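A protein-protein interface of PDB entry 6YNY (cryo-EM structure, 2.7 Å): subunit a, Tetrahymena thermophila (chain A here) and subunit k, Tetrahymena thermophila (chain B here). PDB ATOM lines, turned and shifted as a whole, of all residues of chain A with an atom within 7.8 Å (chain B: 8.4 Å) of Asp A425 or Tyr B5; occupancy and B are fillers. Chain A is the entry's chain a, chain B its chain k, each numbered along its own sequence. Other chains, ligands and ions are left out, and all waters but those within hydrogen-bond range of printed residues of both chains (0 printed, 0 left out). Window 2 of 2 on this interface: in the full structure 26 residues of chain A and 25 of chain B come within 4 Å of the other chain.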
ATOM      1  N   LYS A 422      29.573 -20.025   1.461  1.00  0.00           N
ATOM      2  CA  LYS A 422      29.969 -19.889   0.072  1.00  0.00           C
ATOM      3  C   LYS A 422      29.603 -18.508  -0.452  1.00  0.00           C
ATOM      4  O   LYS A 422      28.741 -17.816   0.094  1.00  0.00           O
ATOM      5  CB  LYS A 422      29.312 -20.965  -0.791  1.00  0.00           C
ATOM      6  CG  LYS A 422      27.821 -21.061  -0.624  1.00  0.00           C
ATOM      7  CD  LYS A 422      27.227 -22.051  -1.600  1.00  0.00           C
ATOM      8  CE  LYS A 422      27.674 -23.463  -1.296  1.00  0.00           C
ATOM      9  NZ  LYS A 422      27.054 -24.454  -2.206  1.00  0.00           N
ATOM     10  N   HIS A 423      30.292 -18.115  -1.523  1.00  0.00           N
ATOM     11  CA  HIS A 423      30.084 -16.831  -2.172  1.00  0.00           C
ATOM     12  C   HIS A 423      29.390 -16.930  -3.520  1.00  0.00           C
ATOM     13  O   HIS A 423      28.918 -15.909  -4.026  1.00  0.00           O
ATOM     14  CB  HIS A 423      31.426 -16.118  -2.377  1.00  0.00           C
ATOM     15  CG  HIS A 423      32.183 -15.866  -1.113  1.00  0.00           C
ATOM     16  ND1 HIS A 423      32.426 -14.599  -0.631  1.00  0.00           N
ATOM     17  CD2 HIS A 423      32.757 -16.719  -0.233  1.00  0.00           C
ATOM     18  CE1 HIS A 423      33.116 -14.682   0.492  1.00  0.00           C
ATOM     19  NE2 HIS A 423      33.328 -15.958   0.755  1.00  0.00           N
ATOM     20  N   GLU A 424      29.323 -18.121  -4.112  1.00  0.00           N
ATOM     21  CA  GLU A 424      28.754 -18.299  -5.440  1.00  0.00           C
ATOM     22  C   GLU A 424      28.251 -19.726  -5.579  1.00  0.00           C
ATOM     23  O   GLU A 424      28.944 -20.668  -5.183  1.00  0.00           O
ATOM     24  CB  GLU A 424      29.794 -17.988  -6.517  1.00  0.00           C
ATOM     25  CG  GLU A 424      31.060 -18.810  -6.394  1.00  0.00           C
ATOM     26  CD  GLU A 424      32.246 -18.154  -7.065  1.00  0.00           C
ATOM     27  OE1 GLU A 424      33.392 -18.523  -6.740  1.00  0.00           O
ATOM     28  OE2 GLU A 424      32.030 -17.267  -7.915  1.00  0.00           O
ATOM     29  N   ASP A 425      27.048 -19.882  -6.131  1.00  0.00           N
ATOM     30  CA  ASP A 425      26.372 -21.172  -6.183  1.00  0.00           C
ATOM     31  C   ASP A 425      25.734 -21.408  -7.547  1.00  0.00           C
ATOM     32  O   ASP A 425      24.595 -21.872  -7.642  1.00  0.00           O
ATOM     33  CB  ASP A 425      25.320 -21.272  -5.079  1.00  0.00           C
ATOM     34  CG  ASP A 425      24.284 -20.166  -5.160  1.00  0.00           C
ATOM     35  OD1 ASP A 425      23.543 -20.105  -6.164  1.00  0.00           O
ATOM     36  OD2 ASP A 425      24.211 -19.353  -4.216  1.00  0.00           O
ATOM     37  N   PHE A 426      26.454 -21.105  -8.626  1.00  0.00           N
ATOM     38  CA  PHE A 426      25.858 -21.192  -9.953  1.00  0.00           C
ATOM     39  C   PHE A 426      25.930 -22.582 -10.573  1.00  0.00           C
ATOM     40  O   PHE A 426      25.304 -22.803 -11.613  1.00  0.00           O
ATOM     41  CB  PHE A 426      26.494 -20.166 -10.903  1.00  0.00           C
ATOM     42  CG  PHE A 426      27.917 -20.450 -11.274  1.00  0.00           C
ATOM     43  CD1 PHE A 426      28.956 -19.828 -10.614  1.00  0.00           C
ATOM     44  CD2 PHE A 426      28.215 -21.300 -12.321  1.00  0.00           C
ATOM     45  CE1 PHE A 426      30.260 -20.071 -10.968  1.00  0.00           C
ATOM     46  CE2 PHE A 426      29.517 -21.547 -12.676  1.00  0.00           C
ATOM     47  CZ  PHE A 426      30.542 -20.929 -12.000  1.00  0.00           C
ATOM     48  N   PHE A 427      26.656 -23.526  -9.974  1.00  0.00           N
ATOM     49  CA  PHE A 427      26.613 -24.900 -10.469  1.00  0.00           C
ATOM     50  C   PHE A 427      25.291 -25.574 -10.131  1.00  0.00           C
ATOM     51  O   PHE A 427      24.766 -26.356 -10.929  1.00  0.00           O
ATOM     52  CB  PHE A 427      27.769 -25.716  -9.889  1.00  0.00           C
ATOM     53  CG  PHE A 427      29.072 -25.586 -10.637  1.00  0.00           C
ATOM     54  CD1 PHE A 427      29.162 -24.905 -11.836  1.00  0.00           C
ATOM     55  CD2 PHE A 427      30.214 -26.168 -10.130  1.00  0.00           C
ATOM     56  CE1 PHE A 427      30.358 -24.805 -12.499  1.00  0.00           C
ATOM     57  CE2 PHE A 427      31.410 -26.070 -10.793  1.00  0.00           C
ATOM     58  CZ  PHE A 427      31.482 -25.386 -11.976  1.00  0.00           C
ATOM     59  N   SER A 428      24.742 -25.291  -8.951  1.00  0.00           N
ATOM     60  CA  SER A 428      23.525 -25.973  -8.526  1.00  0.00           C
ATOM     61  C   SER A 428      22.375 -25.705  -9.486  1.00  0.00           C
ATOM     62  O   SER A 428      21.617 -26.619  -9.827  1.00  0.00           O
ATOM     63  CB  SER A 428      23.152 -25.534  -7.113  1.00  0.00           C
ATOM     64  OG  SER A 428      22.865 -24.149  -7.075  1.00  0.00           O
ATOM     65  N   LYS A 429      22.233 -24.459  -9.935  1.00  0.00           N
ATOM     66  CA  LYS A 429      21.097 -24.094 -10.769  1.00  0.00           C
ATOM     67  C   LYS A 429      21.315 -24.428 -12.237  1.00  0.00           C
ATOM     68  O   LYS A 429      20.345 -24.693 -12.954  1.00  0.00           O
ATOM     69  CB  LYS A 429      20.801 -22.607 -10.602  1.00  0.00           C
ATOM     70  CG  LYS A 429      20.081 -22.290  -9.307  1.00  0.00           C
ATOM     71  CD  LYS A 429      19.727 -20.824  -9.194  1.00  0.00           C
ATOM     72  CE  LYS A 429      20.948 -19.975  -8.934  1.00  0.00           C
ATOM     73  NZ  LYS A 429      20.571 -18.564  -8.675  1.00  0.00           N
ATOM     74  N   LYS A 430      22.563 -24.426 -12.704  1.00  0.00           N
ATOM     75  CA  LYS A 430      22.823 -24.796 -14.090  1.00  0.00           C
ATOM     76  C   LYS A 430      22.590 -26.283 -14.317  1.00  0.00           C
ATOM     77  O   LYS A 430      22.123 -26.686 -15.388  1.00  0.00           O
ATOM     78  CB  LYS A 430      24.250 -24.422 -14.470  1.00  0.00           C
ATOM     79  CG  LYS A 430      24.558 -22.946 -14.392  1.00  0.00           C
ATOM     80  CD  LYS A 430      24.038 -22.182 -15.581  1.00  0.00           C
ATOM     81  CE  LYS A 430      24.588 -20.769 -15.594  1.00  0.00           C
ATOM     82  NZ  LYS A 430      24.133 -19.999 -16.778  1.00  0.00           N
ATOM     83  N   GLU A 433      18.812 -26.778 -14.856  1.00  0.00           N
ATOM     84  CA  GLU A 433      18.382 -26.400 -16.196  1.00  0.00           C
ATOM     85  C   GLU A 433      18.921 -27.366 -17.240  1.00  0.00           C
ATOM     86  O   GLU A 433      18.233 -27.688 -18.215  1.00  0.00           O
ATOM     87  CB  GLU A 433      18.837 -24.975 -16.500  1.00  0.00           C
ATOM     88  CG  GLU A 433      18.407 -24.458 -17.855  1.00  0.00           C
ATOM     89  CD  GLU A 433      18.863 -23.035 -18.103  1.00  0.00           C
ATOM     90  OE1 GLU A 433      19.638 -22.506 -17.278  1.00  0.00           O
ATOM     91  OE2 GLU A 433      18.447 -22.444 -19.121  1.00  0.00           O
ATOM     92  N   MET B   1      24.648 -10.909 -14.656  1.00  0.00           N
ATOM     93  CA  MET B   1      23.811 -11.561 -13.619  1.00  0.00           C
ATOM     94  C   MET B   1      24.666 -12.292 -12.598  1.00  0.00           C
ATOM     95  O   MET B   1      24.273 -13.339 -12.088  1.00  0.00           O
ATOM     96  CB  MET B   1      22.832 -12.538 -14.267  1.00  0.00           C
ATOM     97  CG  MET B   1      23.488 -13.596 -15.125  1.00  0.00           C
ATOM     98  SD  MET B   1      22.367 -14.941 -15.534  1.00  0.00           S
ATOM     99  CE  MET B   1      20.981 -14.024 -16.188  1.00  0.00           C
ATOM    100  N   TRP B   2      25.841 -11.740 -12.299  1.00  0.00           N
ATOM    101  CA  TRP B   2      26.705 -12.373 -11.314  1.00  0.00           C
ATOM    102  C   TRP B   2      26.135 -12.244  -9.909  1.00  0.00           C
ATOM    103  O   TRP B   2      26.359 -13.120  -9.068  1.00  0.00           O
ATOM    104  CB  TRP B   2      28.111 -11.782 -11.381  1.00  0.00           C
ATOM    105  CG  TRP B   2      28.191 -10.335 -11.048  1.00  0.00           C
ATOM    106  CD1 TRP B   2      28.193  -9.296 -11.925  1.00  0.00           C
ATOM    107  CD2 TRP B   2      28.292  -9.760  -9.743  1.00  0.00           C
ATOM    108  NE1 TRP B   2      28.286  -8.108 -11.249  1.00  0.00           N
ATOM    109  CE2 TRP B   2      28.348  -8.366  -9.906  1.00  0.00           C
ATOM    110  CE3 TRP B   2      28.338 -10.289  -8.452  1.00  0.00           C
ATOM    111  CZ2 TRP B   2      28.447  -7.496  -8.831  1.00  0.00           C
ATOM    112  CZ3 TRP B   2      28.435  -9.423  -7.389  1.00  0.00           C
ATOM    113  CH2 TRP B   2      28.489  -8.042  -7.584  1.00  0.00           C
ATOM    114  N   TYR B   3      25.398 -11.166  -9.641  1.00  0.00           N
ATOM    115  CA  TYR B   3      24.748 -11.018  -8.345  1.00  0.00           C
ATOM    116  C   TYR B   3      23.617 -12.020  -8.167  1.00  0.00           C
ATOM    117  O   TYR B   3      23.278 -12.373  -7.033  1.00  0.00           O
ATOM    118  CB  TYR B   3      24.234  -9.589  -8.195  1.00  0.00           C
ATOM    119  CG  TYR B   3      23.493  -9.322  -6.910  1.00  0.00           C
ATOM    120  CD1 TYR B   3      24.175  -9.085  -5.729  1.00  0.00           C
ATOM    121  CD2 TYR B   3      22.110  -9.293  -6.881  1.00  0.00           C
ATOM    122  CE1 TYR B   3      23.500  -8.839  -4.556  1.00  0.00           C
ATOM    123  CE2 TYR B   3      21.429  -9.049  -5.715  1.00  0.00           C
ATOM    124  CZ  TYR B   3      22.128  -8.822  -4.555  1.00  0.00           C
ATOM    125  OH  TYR B   3      21.446  -8.577  -3.389  1.00  0.00           O
ATOM    126  N   LYS B   4      23.026 -12.489  -9.266  1.00  0.00           N
ATOM    127  CA  LYS B   4      22.017 -13.536  -9.170  1.00  0.00           C
ATOM    128  C   LYS B   4      22.597 -14.801  -8.558  1.00  0.00           C
ATOM    129  O   LYS B   4      21.911 -15.514  -7.817  1.00  0.00           O
ATOM    130  CB  LYS B   4      21.449 -13.831 -10.554  1.00  0.00           C
ATOM    131  CG  LYS B   4      20.451 -14.964 -10.598  1.00  0.00           C
ATOM    132  CD  LYS B   4      20.045 -15.263 -12.017  1.00  0.00           C
ATOM    133  CE  LYS B   4      19.055 -16.405 -12.085  1.00  0.00           C
ATOM    134  NZ  LYS B   4      18.609 -16.663 -13.481  1.00  0.00           N
ATOM    135  N   TYR B   5      23.855 -15.099  -8.862  1.00  0.00           N
ATOM    136  CA  TYR B   5      24.531 -16.275  -8.342  1.00  0.00           C
ATOM    137  C   TYR B   5      25.395 -15.966  -7.128  1.00  0.00           C
ATOM    138  O   TYR B   5      26.135 -16.840  -6.670  1.00  0.00           O
ATOM    139  CB  TYR B   5      25.375 -16.919  -9.438  1.00  0.00           C
ATOM    140  CG  TYR B   5      24.574 -17.320 -10.652  1.00  0.00           C
ATOM    141  CD1 TYR B   5      23.714 -18.403 -10.607  1.00  0.00           C
ATOM    142  CD2 TYR B   5      24.682 -16.622 -11.841  1.00  0.00           C
ATOM    143  CE1 TYR B   5      22.981 -18.774 -11.706  1.00  0.00           C
ATOM    144  CE2 TYR B   5      23.951 -16.988 -12.947  1.00  0.00           C
ATOM    145  CZ  TYR B   5      23.103 -18.065 -12.873  1.00  0.00           C
ATOM    146  OH  TYR B   5      22.372 -18.434 -13.975  1.00  0.00           O
ATOM    147  N   PHE B   6      25.324 -14.748  -6.602  1.00  0.00           N
ATOM    148  CA  PHE B   6      26.032 -14.414  -5.377  1.00  0.00           C
ATOM    149  C   PHE B   6      25.246 -14.922  -4.176  1.00  0.00           C
ATOM    150  O   PHE B   6      24.028 -14.740  -4.097  1.00  0.00           O
ATOM    151  CB  PHE B   6      26.243 -12.906  -5.274  1.00  0.00           C
ATOM    152  CG  PHE B   6      26.763 -12.459  -3.943  1.00  0.00           C
ATOM    153  CD1 PHE B   6      28.115 -12.482  -3.669  1.00  0.00           C
ATOM    154  CD2 PHE B   6      25.897 -12.011  -2.964  1.00  0.00           C
ATOM    155  CE1 PHE B   6      28.591 -12.074  -2.445  1.00  0.00           C
ATOM    156  CE2 PHE B   6      26.371 -11.601  -1.742  1.00  0.00           C
ATOM    157  CZ  PHE B   6      27.718 -11.632  -1.483  1.00  0.00           C
ATOM    158  N   SER B   7      25.945 -15.559  -3.246  1.00  0.00           N
ATOM    159  CA  SER B   7      25.334 -16.132  -2.056  1.00  0.00           C
ATOM    160  C   SER B   7      25.453 -15.135  -0.913  1.00  0.00           C
ATOM    161  O   SER B   7      26.564 -14.772  -0.515  1.00  0.00           O
ATOM    162  CB  SER B   7      25.997 -17.455  -1.689  1.00  0.00           C
ATOM    163  OG  SER B   7      25.219 -18.166  -0.746  1.00  0.00           O
ATOM    164  N   LYS B   8      24.310 -14.699  -0.385  1.00  0.00           N
ATOM    165  CA  LYS B   8      24.321 -13.709   0.682  1.00  0.00           C
ATOM    166  C   LYS B   8      24.776 -14.286   2.014  1.00  0.00           C
ATOM    167  O   LYS B   8      24.951 -13.523   2.968  1.00  0.00           O
ATOM    168  CB  LYS B   8      22.937 -13.091   0.847  1.00  0.00           C
ATOM    169  CG  LYS B   8      22.402 -12.425  -0.399  1.00  0.00           C
ATOM    170  CD  LYS B   8      21.109 -11.703  -0.112  1.00  0.00           C
ATOM    171  CE  LYS B   8      20.536 -11.067  -1.355  1.00  0.00           C
ATOM    172  NZ  LYS B   8      20.061 -12.090  -2.323  1.00  0.00           N
ATOM    173  N   GLN B   9      24.969 -15.601   2.109  1.00  0.00           N
ATOM    174  CA  GLN B   9      25.458 -16.175   3.352  1.00  0.00           C
ATOM    175  C   GLN B   9      26.897 -15.777   3.642  1.00  0.00           C
ATOM    176  O   GLN B   9      27.385 -16.046   4.743  1.00  0.00           O
ATOM    177  CB  GLN B   9      25.334 -17.698   3.319  1.00  0.00           C
ATOM    178  CG  GLN B   9      26.246 -18.379   2.338  1.00  0.00           C
ATOM    179  CD  GLN B   9      26.029 -19.879   2.287  1.00  0.00           C
ATOM    180  OE1 GLN B   9      26.966 -20.659   2.452  1.00  0.00           O
ATOM    181  NE2 GLN B   9      24.794 -20.289   2.054  1.00  0.00           N
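Of the 10 printed residues of chain A, 7 touch a printed residue of chain B.
Printed residues of chain A that touch a printed residue of chain B: Lys A422, His A423, Glu A424, Asp A425, Phe A426, Lys A429 and Lys A430.
Hydrophobic or aromatic side chains of chain A within 4 Å of the printed part of chain B: Phe A426.
Of the 9 printed residues of chain B, 5 touch a printed residue of chain A.
Hydrophobic or aromatic side chains of chain B that line the printed part of chain A: Tyr B5 and Phe B6.
O of Lys A422 touches CB of Ser B7 (3.3 Å).
His A423 touches Tyr B5.
Phe B6 touches His A423.
Tyr B5 touches Glu A424.
Asp A425 touches Ser B7.
Phe A426 touches Tyr B5 (CB to CD1, 3.3 Å).
Tyr B5 touches Lys A429.
Lys A430 touches Tyr B5.
O of His A423 is in hydrogen-bond range of N of Ser B7, 3.1 Å away.
The backbone NH (N) of Asp A425 lies within hydrogen-bond range of the backbone carbonyl oxygen (O) of Tyr B5 (3.2 Å).
The side-chain amide oxygen (OE1) of Gln B9 is in hydrogen-bond range of the backbone NH (N) of Lys A422, at 2.9 Å.
O of Lys B4 sits at hydrogen-bond distance from NZ of Lys A429.
The side-chain hydroxyl (OG) of Ser A428 lies within hydrogen-bond range of the backbone carbonyl oxygen (O) of Asp A425 (2.9 Å).
Asp A425 touches just these residues of chain B: Tyr B5 and Ser B7.
Of the printed residues of chain B, Phe A426 touches Tyr B5 (3.3 Å).
Of the printed residues of chain B, Lys A429 touches Lys B4 and Tyr B5.
Tyr B3 touches none of the printed residues of chain A.
Tyr B5 touches six residues of chain A.
Of the printed residues of chain A, Gln B9 touches Lys A422 (2.9 Å).
The nearest residue of chain B that does not touch Asp A425 is Phe B6 (4.6 Å).
The nearest printed residue of chain A that does not touch Tyr B5 is Glu A433 (5.9 Å).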
